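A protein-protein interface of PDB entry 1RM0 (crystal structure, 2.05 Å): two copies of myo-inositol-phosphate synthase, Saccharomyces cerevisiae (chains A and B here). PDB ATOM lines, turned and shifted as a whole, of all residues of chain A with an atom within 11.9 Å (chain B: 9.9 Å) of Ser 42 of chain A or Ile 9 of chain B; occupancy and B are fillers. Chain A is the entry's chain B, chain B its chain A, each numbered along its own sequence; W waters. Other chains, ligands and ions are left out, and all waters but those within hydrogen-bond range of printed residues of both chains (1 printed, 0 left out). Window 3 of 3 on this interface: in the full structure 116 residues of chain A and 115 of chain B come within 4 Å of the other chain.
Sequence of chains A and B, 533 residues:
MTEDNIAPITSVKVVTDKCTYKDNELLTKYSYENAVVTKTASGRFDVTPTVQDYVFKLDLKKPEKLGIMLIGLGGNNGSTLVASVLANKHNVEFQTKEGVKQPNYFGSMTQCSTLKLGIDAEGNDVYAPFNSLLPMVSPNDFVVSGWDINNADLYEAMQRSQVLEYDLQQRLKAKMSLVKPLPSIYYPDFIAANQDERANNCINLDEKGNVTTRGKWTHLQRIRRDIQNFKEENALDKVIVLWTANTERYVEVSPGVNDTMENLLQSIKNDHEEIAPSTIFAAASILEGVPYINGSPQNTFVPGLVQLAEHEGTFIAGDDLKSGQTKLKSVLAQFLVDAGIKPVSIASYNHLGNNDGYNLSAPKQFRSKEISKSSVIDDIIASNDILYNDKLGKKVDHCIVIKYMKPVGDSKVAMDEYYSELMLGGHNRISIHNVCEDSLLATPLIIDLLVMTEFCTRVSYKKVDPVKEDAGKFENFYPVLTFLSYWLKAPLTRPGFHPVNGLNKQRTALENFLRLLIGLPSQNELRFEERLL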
ATOM      1  N   THR A  38      -7.031   1.737   2.272  1.00  0.00           N
ATOM      2  CA  THR A  38      -7.167   0.333   1.903  1.00  0.00           C
ATOM      3  C   THR A  38      -5.748  -0.232   1.827  1.00  0.00           C
ATOM      4  O   THR A  38      -4.802   0.494   1.520  1.00  0.00           O
ATOM      5  CB  THR A  38      -7.888   0.170   0.546  1.00  0.00           C
ATOM      6  OG1 THR A  38      -7.142   0.825  -0.486  1.00  0.00           O
ATOM      7  CG2 THR A  38      -9.278   0.785   0.617  1.00  0.00           C
ATOM      8  N   LYS A  39      -5.584  -1.514   2.129  1.00  0.00           N
ATOM      9  CA  LYS A  39      -4.249  -2.093   2.091  1.00  0.00           C
ATOM     10  C   LYS A  39      -4.101  -3.172   1.027  1.00  0.00           C
ATOM     11  O   LYS A  39      -4.904  -4.097   0.963  1.00  0.00           O
ATOM     12  CB  LYS A  39      -3.883  -2.679   3.462  1.00  0.00           C
ATOM     13  CG  LYS A  39      -2.414  -3.084   3.572  1.00  0.00           C
ATOM     14  CD  LYS A  39      -2.159  -4.126   4.654  1.00  0.00           C
ATOM     15  CE  LYS A  39      -2.443  -3.594   6.046  1.00  0.00           C
ATOM     16  NZ  LYS A  39      -2.147  -4.626   7.084  1.00  0.00           N
ATOM     17  N   THR A  40      -3.065  -3.046   0.198  1.00  0.00           N
ATOM     18  CA  THR A  40      -2.789  -4.023  -0.852  1.00  0.00           C
ATOM     19  C   THR A  40      -2.148  -5.237  -0.206  1.00  0.00           C
ATOM     20  O   THR A  40      -1.683  -5.167   0.931  1.00  0.00           O
ATOM     21  CB  THR A  40      -1.789  -3.489  -1.895  1.00  0.00           C
ATOM     22  OG1 THR A  40      -2.312  -2.302  -2.499  1.00  0.00           O
ATOM     23  CG2 THR A  40      -1.538  -4.535  -2.980  1.00  0.00           C
ATOM     24  N   ALA A  41      -2.120  -6.348  -0.933  1.00  0.00           N
ATOM     25  CA  ALA A  41      -1.507  -7.569  -0.424  1.00  0.00           C
ATOM     26  C   ALA A  41      -0.012  -7.311  -0.239  1.00  0.00           C
ATOM     27  O   ALA A  41       0.585  -7.722   0.759  1.00  0.00           O
ATOM     28  CB  ALA A  41      -1.729  -8.712  -1.406  1.00  0.00           C
ATOM     29  N   SER A  42       0.577  -6.615  -1.211  1.00  0.00           N
ATOM     30  CA  SER A  42       1.997  -6.276  -1.183  1.00  0.00           C
ATOM     31  C   SER A  42       2.329  -5.448   0.056  1.00  0.00           C
ATOM     32  O   SER A  42       3.500  -5.227   0.376  1.00  0.00           O
ATOM     33  CB  SER A  42       2.373  -5.495  -2.446  1.00  0.00           C
ATOM     34  OG  SER A  42       1.550  -4.351  -2.602  1.00  0.00           O
ATOM     35  N   GLY A  43       1.284  -4.993   0.743  1.00  0.00           N
ATOM     36  CA  GLY A  43       1.465  -4.202   1.944  1.00  0.00           C
ATOM     37  C   GLY A  43       1.553  -2.712   1.687  1.00  0.00           C
ATOM     38  O   GLY A  43       2.227  -1.992   2.425  1.00  0.00           O
ATOM     39  N   ARG A  44       0.884  -2.238   0.642  1.00  0.00           N
ATOM     40  CA  ARG A  44       0.912  -0.814   0.333  1.00  0.00           C
ATOM     41  C   ARG A  44      -0.408  -0.199   0.782  1.00  0.00           C
ATOM     42  O   ARG A  44      -1.475  -0.763   0.553  1.00  0.00           O
ATOM     43  CB  ARG A  44       1.141  -0.606  -1.169  1.00  0.00           C
ATOM     44  CG  ARG A  44       1.409   0.839  -1.598  1.00  0.00           C
ATOM     45  CD  ARG A  44       0.112   1.593  -1.841  1.00  0.00           C
ATOM     46  NE  ARG A  44      -0.759   0.860  -2.759  1.00  0.00           N
ATOM     47  CZ  ARG A  44      -0.515   0.680  -4.053  1.00  0.00           C
ATOM     48  NH1 ARG A  44      -1.368  -0.012  -4.798  1.00  0.00           N
ATOM     49  NH2 ARG A  44       0.570   1.205  -4.607  1.00  0.00           N
ATOM     50  N   PHE A  45      -0.328   0.948   1.446  1.00  0.00           N
ATOM     51  CA  PHE A  45      -1.518   1.627   1.939  1.00  0.00           C
ATOM     52  C   PHE A  45      -1.992   2.701   0.977  1.00  0.00           C
ATOM     53  O   PHE A  45      -1.279   3.673   0.727  1.00  0.00           O
ATOM     54  CB  PHE A  45      -1.237   2.286   3.289  1.00  0.00           C
ATOM     55  CG  PHE A  45      -1.164   1.328   4.436  1.00  0.00           C
ATOM     56  CD1 PHE A  45      -2.319   0.729   4.931  1.00  0.00           C
ATOM     57  CD2 PHE A  45       0.057   1.036   5.038  1.00  0.00           C
ATOM     58  CE1 PHE A  45      -2.259  -0.145   6.012  1.00  0.00           C
ATOM     59  CE2 PHE A  45       0.127   0.165   6.118  1.00  0.00           C
ATOM     60  CZ  PHE A  45      -1.034  -0.427   6.607  1.00  0.00           C
ATOM     61  N   ASP A  46      -3.194   2.530   0.441  1.00  0.00           N
ATOM     62  CA  ASP A  46      -3.754   3.515  -0.468  1.00  0.00           C
ATOM     63  C   ASP A  46      -4.668   4.406   0.335  1.00  0.00           C
ATOM     64  O   ASP A  46      -5.656   3.944   0.908  1.00  0.00           O
ATOM     65  CB  ASP A  46      -4.505   2.831  -1.594  1.00  0.00           C
ATOM     66  CG  ASP A  46      -3.572   2.225  -2.605  1.00  0.00           C
ATOM     67  OD1 ASP A  46      -2.707   2.968  -3.119  1.00  0.00           O
ATOM     68  OD2 ASP A  46      -3.696   1.013  -2.883  1.00  0.00           O
ATOM     69  N   ASP A 385       0.762  -3.485  14.708  1.00  0.00           N
ATOM     70  CA  ASP A 385       1.078  -4.860  14.336  1.00  0.00           C
ATOM     71  C   ASP A 385       2.588  -5.077  14.203  1.00  0.00           C
ATOM     72  O   ASP A 385       3.036  -6.140  13.756  1.00  0.00           O
ATOM     73  CB  ASP A 385       0.361  -5.265  13.040  1.00  0.00           C
ATOM     74  CG  ASP A 385       0.883  -4.534  11.817  1.00  0.00           C
ATOM     75  OD1 ASP A 385       0.412  -4.847  10.703  1.00  0.00           O
ATOM     76  OD2 ASP A 385       1.754  -3.650  11.959  1.00  0.00           O
ATOM     77  N   ILE A 386       3.369  -4.069  14.588  1.00  0.00           N
ATOM     78  CA  ILE A 386       4.822  -4.197  14.554  1.00  0.00           C
ATOM     79  C   ILE A 386       5.160  -4.962  15.824  1.00  0.00           C
ATOM     80  O   ILE A 386       5.966  -5.897  15.811  1.00  0.00           O
ATOM     81  CB  ILE A 386       5.551  -2.832  14.620  1.00  0.00           C
ATOM     82  CG1 ILE A 386       5.208  -1.981  13.393  1.00  0.00           C
ATOM     83  CG2 ILE A 386       7.068  -3.066  14.716  1.00  0.00           C
ATOM     84  CD1 ILE A 386       5.858  -0.618  13.407  1.00  0.00           C
ATOM     85  N   ILE B   9       7.381  -5.248   2.045  1.00  0.00           N
ATOM     86  CA  ILE B   9       7.711  -3.825   2.346  1.00  0.00           C
ATOM     87  C   ILE B   9       6.437  -3.029   2.606  1.00  0.00           C
ATOM     88  O   ILE B   9       5.384  -3.323   2.040  1.00  0.00           O
ATOM     89  CB  ILE B   9       8.477  -3.159   1.171  1.00  0.00           C
ATOM     90  CG1 ILE B   9       9.788  -3.906   0.909  1.00  0.00           C
ATOM     91  CG2 ILE B   9       8.769  -1.696   1.489  1.00  0.00           C
ATOM     92  CD1 ILE B   9      10.754  -3.886   2.076  1.00  0.00           C
ATOM     93  N   THR B  10       6.544  -2.023   3.467  1.00  0.00           N
ATOM     94  CA  THR B  10       5.412  -1.170   3.806  1.00  0.00           C
ATOM     95  C   THR B  10       5.595   0.212   3.183  1.00  0.00           C
ATOM     96  O   THR B  10       6.661   0.822   3.300  1.00  0.00           O
ATOM     97  CB  THR B  10       5.284  -1.003   5.329  1.00  0.00           C
ATOM     98  OG1 THR B  10       5.278  -2.294   5.950  1.00  0.00           O
ATOM     99  CG2 THR B  10       3.996  -0.263   5.679  1.00  0.00           C
ATOM    100  N   SER B  11       4.555   0.699   2.518  1.00  0.00           N
ATOM    101  CA  SER B  11       4.605   2.013   1.888  1.00  0.00           C
ATOM    102  C   SER B  11       3.219   2.623   1.852  1.00  0.00           C
ATOM    103  O   SER B  11       2.208   1.923   1.920  1.00  0.00           O
ATOM    104  CB  SER B  11       5.139   1.915   0.460  1.00  0.00           C
ATOM    105  OG  SER B  11       4.222   1.227  -0.374  1.00  0.00           O
ATOM    106  N   VAL B  12       3.180   3.939   1.733  1.00  0.00           N
ATOM    107  CA  VAL B  12       1.917   4.640   1.684  1.00  0.00           C
ATOM    108  C   VAL B  12       1.807   5.447   0.390  1.00  0.00           C
ATOM    109  O   VAL B  12       2.776   6.072  -0.051  1.00  0.00           O
ATOM    110  CB  VAL B  12       1.779   5.573   2.896  1.00  0.00           C
ATOM    111  CG1 VAL B  12       0.407   6.218   2.901  1.00  0.00           C
ATOM    112  CG2 VAL B  12       1.999   4.783   4.179  1.00  0.00           C
ATOM    113  N   LYS B  13       0.626   5.411  -0.221  1.00  0.00           N
ATOM    114  CA  LYS B  13       0.356   6.138  -1.456  1.00  0.00           C
ATOM    115  C   LYS B  13      -0.867   7.033  -1.230  1.00  0.00           C
ATOM    116  O   LYS B  13      -1.995   6.549  -1.152  1.00  0.00           O
ATOM    117  CB  LYS B  13       0.095   5.147  -2.595  1.00  0.00           C
ATOM    118  CG  LYS B  13      -0.390   5.774  -3.897  1.00  0.00           C
ATOM    119  CD  LYS B  13       0.552   6.860  -4.402  1.00  0.00           C
ATOM    120  CE  LYS B  13       0.118   7.378  -5.771  1.00  0.00           C
ATOM    121  NZ  LYS B  13      -1.275   7.919  -5.772  1.00  0.00           N
ATOM    122  N   LYS B  62      17.492   8.703   0.121  1.00  0.00           N
ATOM    123  CA  LYS B  62      18.080   8.543   1.447  1.00  0.00           C
ATOM    124  C   LYS B  62      19.420   7.823   1.281  1.00  0.00           C
ATOM    125  O   LYS B  62      19.585   7.029   0.355  1.00  0.00           O
ATOM    126  CB  LYS B  62      17.147   7.732   2.349  1.00  0.00           C
ATOM    127  CG  LYS B  62      16.857   6.333   1.859  1.00  0.00           C
ATOM    128  CD  LYS B  62      15.985   5.593   2.858  1.00  0.00           C
ATOM    129  CE  LYS B  62      15.751   4.164   2.430  1.00  0.00           C
ATOM    130  NZ  LYS B  62      14.957   3.420   3.449  1.00  0.00           N
ATOM    131  N   ALA B 128      -0.240   2.645  10.230  1.00  0.00           N
ATOM    132  CA  ALA B 128       0.915   2.222   9.449  1.00  0.00           C
ATOM    133  C   ALA B 128       2.191   2.584  10.222  1.00  0.00           C
ATOM    134  O   ALA B 128       2.197   3.502  11.051  1.00  0.00           O
ATOM    135  CB  ALA B 128       0.908   2.903   8.082  1.00  0.00           C
ATOM    136  N   PRO B 129       3.285   1.854   9.973  1.00  0.00           N
ATOM    137  CA  PRO B 129       4.521   2.168  10.685  1.00  0.00           C
ATOM    138  C   PRO B 129       4.919   3.637  10.544  1.00  0.00           C
ATOM    139  O   PRO B 129       4.759   4.237   9.478  1.00  0.00           O
ATOM    140  CB  PRO B 129       5.536   1.231  10.036  1.00  0.00           C
ATOM    141  CG  PRO B 129       4.710   0.034   9.706  1.00  0.00           C
ATOM    142  CD  PRO B 129       3.453   0.659   9.128  1.00  0.00           C
ATOM    143  N   ASN B 131       7.691   4.793  10.258  1.00  0.00           N
ATOM    144  CA  ASN B 131       8.701   4.938   9.236  1.00  0.00           C
ATOM    145  C   ASN B 131       8.272   4.432   7.872  1.00  0.00           C
ATOM    146  O   ASN B 131       9.119   4.183   7.020  1.00  0.00           O
ATOM    147  CB  ASN B 131       9.987   4.227   9.677  1.00  0.00           C
ATOM    148  CG  ASN B 131       9.832   2.719   9.744  1.00  0.00           C
ATOM    149  OD1 ASN B 131       8.753   2.183   9.518  1.00  0.00           O
ATOM    150  ND2 ASN B 131      10.921   2.026  10.057  1.00  0.00           N
ATOM    151  N   SER B 132       6.970   4.284   7.646  1.00  0.00           N
ATOM    152  CA  SER B 132       6.506   3.796   6.349  1.00  0.00           C
ATOM    153  C   SER B 132       5.856   4.893   5.510  1.00  0.00           C
ATOM    154  O   SER B 132       5.562   4.683   4.332  1.00  0.00           O
ATOM    155  CB  SER B 132       5.519   2.637   6.525  1.00  0.00           C
ATOM    156  OG  SER B 132       4.297   3.083   7.085  1.00  0.00           O
ATOM    157  N   LEU B 133       5.635   6.064   6.103  1.00  0.00           N
ATOM    158  CA  LEU B 133       5.030   7.165   5.362  1.00  0.00           C
ATOM    159  C   LEU B 133       5.998   7.711   4.316  1.00  0.00           C
ATOM    160  O   LEU B 133       5.672   7.769   3.133  1.00  0.00           O
ATOM    161  CB  LEU B 133       4.594   8.275   6.322  1.00  0.00           C
ATOM    162  CG  LEU B 133       3.296   8.046   7.120  1.00  0.00           C
ATOM    163  CD1 LEU B 133       3.333   6.709   7.879  1.00  0.00           C
ATOM    164  CD2 LEU B 133       3.092   9.213   8.085  1.00  0.00           C
ATOM    165  N   PRO B 135      10.425   7.844   3.083  1.00  0.00           N
ATOM    166  CA  PRO B 135      11.734   7.191   3.216  1.00  0.00           C
ATOM    167  C   PRO B 135      12.604   7.680   4.371  1.00  0.00           C
ATOM    168  O   PRO B 135      12.952   8.856   4.453  1.00  0.00           O
ATOM    169  CB  PRO B 135      12.381   7.450   1.856  1.00  0.00           C
ATOM    170  CG  PRO B 135      11.840   8.795   1.497  1.00  0.00           C
ATOM    171  CD  PRO B 135      10.371   8.636   1.840  1.00  0.00           C
HETATM  172  O   HOH W   1      -3.265   5.942  -3.473  1.00  0.00           O
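The backbone carbonyl oxygen (O) of Ser 42 of chain A sits close to the backbone carbonyl oxygen (O) of Ile 9 of chain B (3.2 Å).
The backbone NH (N) of Lys 13 of chain B is in hydrogen-bond range of the backbone carbonyl oxygen (O) of Phe 45 of chain A.
The backbone carbonyl oxygen (O) of Ile 9 of chain B sits close to the backbone carbonyl oxygen (O) of Gly 43 of chain A (3.4 Å).
The backbone carbonyl oxygen (O) of Ser 11 of chain B lies within hydrogen-bond range of the backbone NH (N) of Phe 45 of chain A, at 2.8 Å.
Lys 39 of chain A touches none of the printed residues of chain B.
No residue of chain B comes within 4 Å of Ala 41 of chain A.
Ser 42 of chain A touches one residue of chain B.
Gly 43 of chain A touches three residues of chain B.
Of the printed residues of chain B, Phe 45 of chain A touches Thr 10, Ser 11, Val 12, Lys 13 and Ala 128.
Printed residues of chain B within 4 Å of Ile 386 of chain A: Pro 129.
Of chain A, only Ser 42 (3.2 Å) and Gly 43 (3.4 Å) come within 4 Å of Ile 9 of chain B.
Of chain A, only Gly 43 and Phe 45 come within 4 Å of Thr 10 of chain B.
Printed residues of chain A within 4 Å of Lys 13 of chain B: Arg 44 (3.6 Å), Phe 45 (2.7 Å) and Asp 46 (3.6 Å).
Printed residues of chain A within 4 Å of Ala 128 of chain B: Phe 45.
Leu 133 of chain B touches none of the printed residues of chain A.
The nearest residue of chain B that does not touch Ser 42 of chain A is Thr 10 of chain B (5.4 Å).
The nearest residue of chain A that does not touch Ile 9 of chain B is Arg 44 of chain A (4.8 Å).
The nearest printed residue of chain B that does not touch Arg 44 of chain A is Val 12 of chain B (4.8 Å).
No position is printed for both chains.
OG1 of Thr 40 of chain A is in hydrogen-bond range of NH1 of Arg 44 of chain A, 3.4 Å away.
The side-chain hydroxyl of Ser 132 of chain B is in hydrogen-bond range of the backbone carbonyl oxygen of Pro 129 of chain B, at 2.7 Å.
The backbone carbonyl oxygen of Thr 38 of chain A is in hydrogen-bond range of the backbone NH of Asp 46 of chain A, 2.8 Å away.
NE of Arg 44 of chain A lies within salt-bridge range of OD1 of Asp 46 of chain A (2.9 Å).
Of the 11 printed residues of chain A, 6 touch a printed residue of chain B.
Printed residues of chain A that touch a printed residue of chain B: Ser 42, Gly 43, Arg 44, Phe 45, Asp 46 and Ile 386.
Of the 12 printed residues of chain B, 7 touch a printed residue of chain A.
Printed residues of chain B that touch a printed residue of chain A: Ile 9, Thr 10, Ser 11, Val 12, Lys 13, Ala 128 and Pro 129.
Hydrophobic or aromatic side chains of chain B that line the printed part of chain A: Val 12, Ala 128 and Pro 129.
Among the printed residues, 13 pairs touch across the chains.
Among the printed residues, no Asp or Glu carboxylate lies within 4 Å of a Lys or Arg side-chain nitrogen of the other chain.
Among the printed residues, pairs that only touch across the chains: Gly 43 of chain A with Thr 10 of chain B (3.6 Å), Gly 43 of chain A with Ser 11 of chain B (3.6 Å), Arg 44 of chain A with Ser 11 of chain B (3.1 Å), Arg 44 of chain A with Lys 13 of chain B (3.6 Å), Phe 45 of chain A with Thr 10 of chain B (3.9 Å), Phe 45 of chain A with Val 12 of chain B (3.5 Å), Phe 45 of chain A with Ala 128 of chain B (3.5 Å), Asp 46 of chain A with Lys 13 of chain B (3.6 Å) and Ile 386 of chain A with Pro 129 of chain B (3.9 Å).
Water W1 lies within hydrogen-bond range of O of Lys 13 of chain B and OD1 of Asp 46 of chain A.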
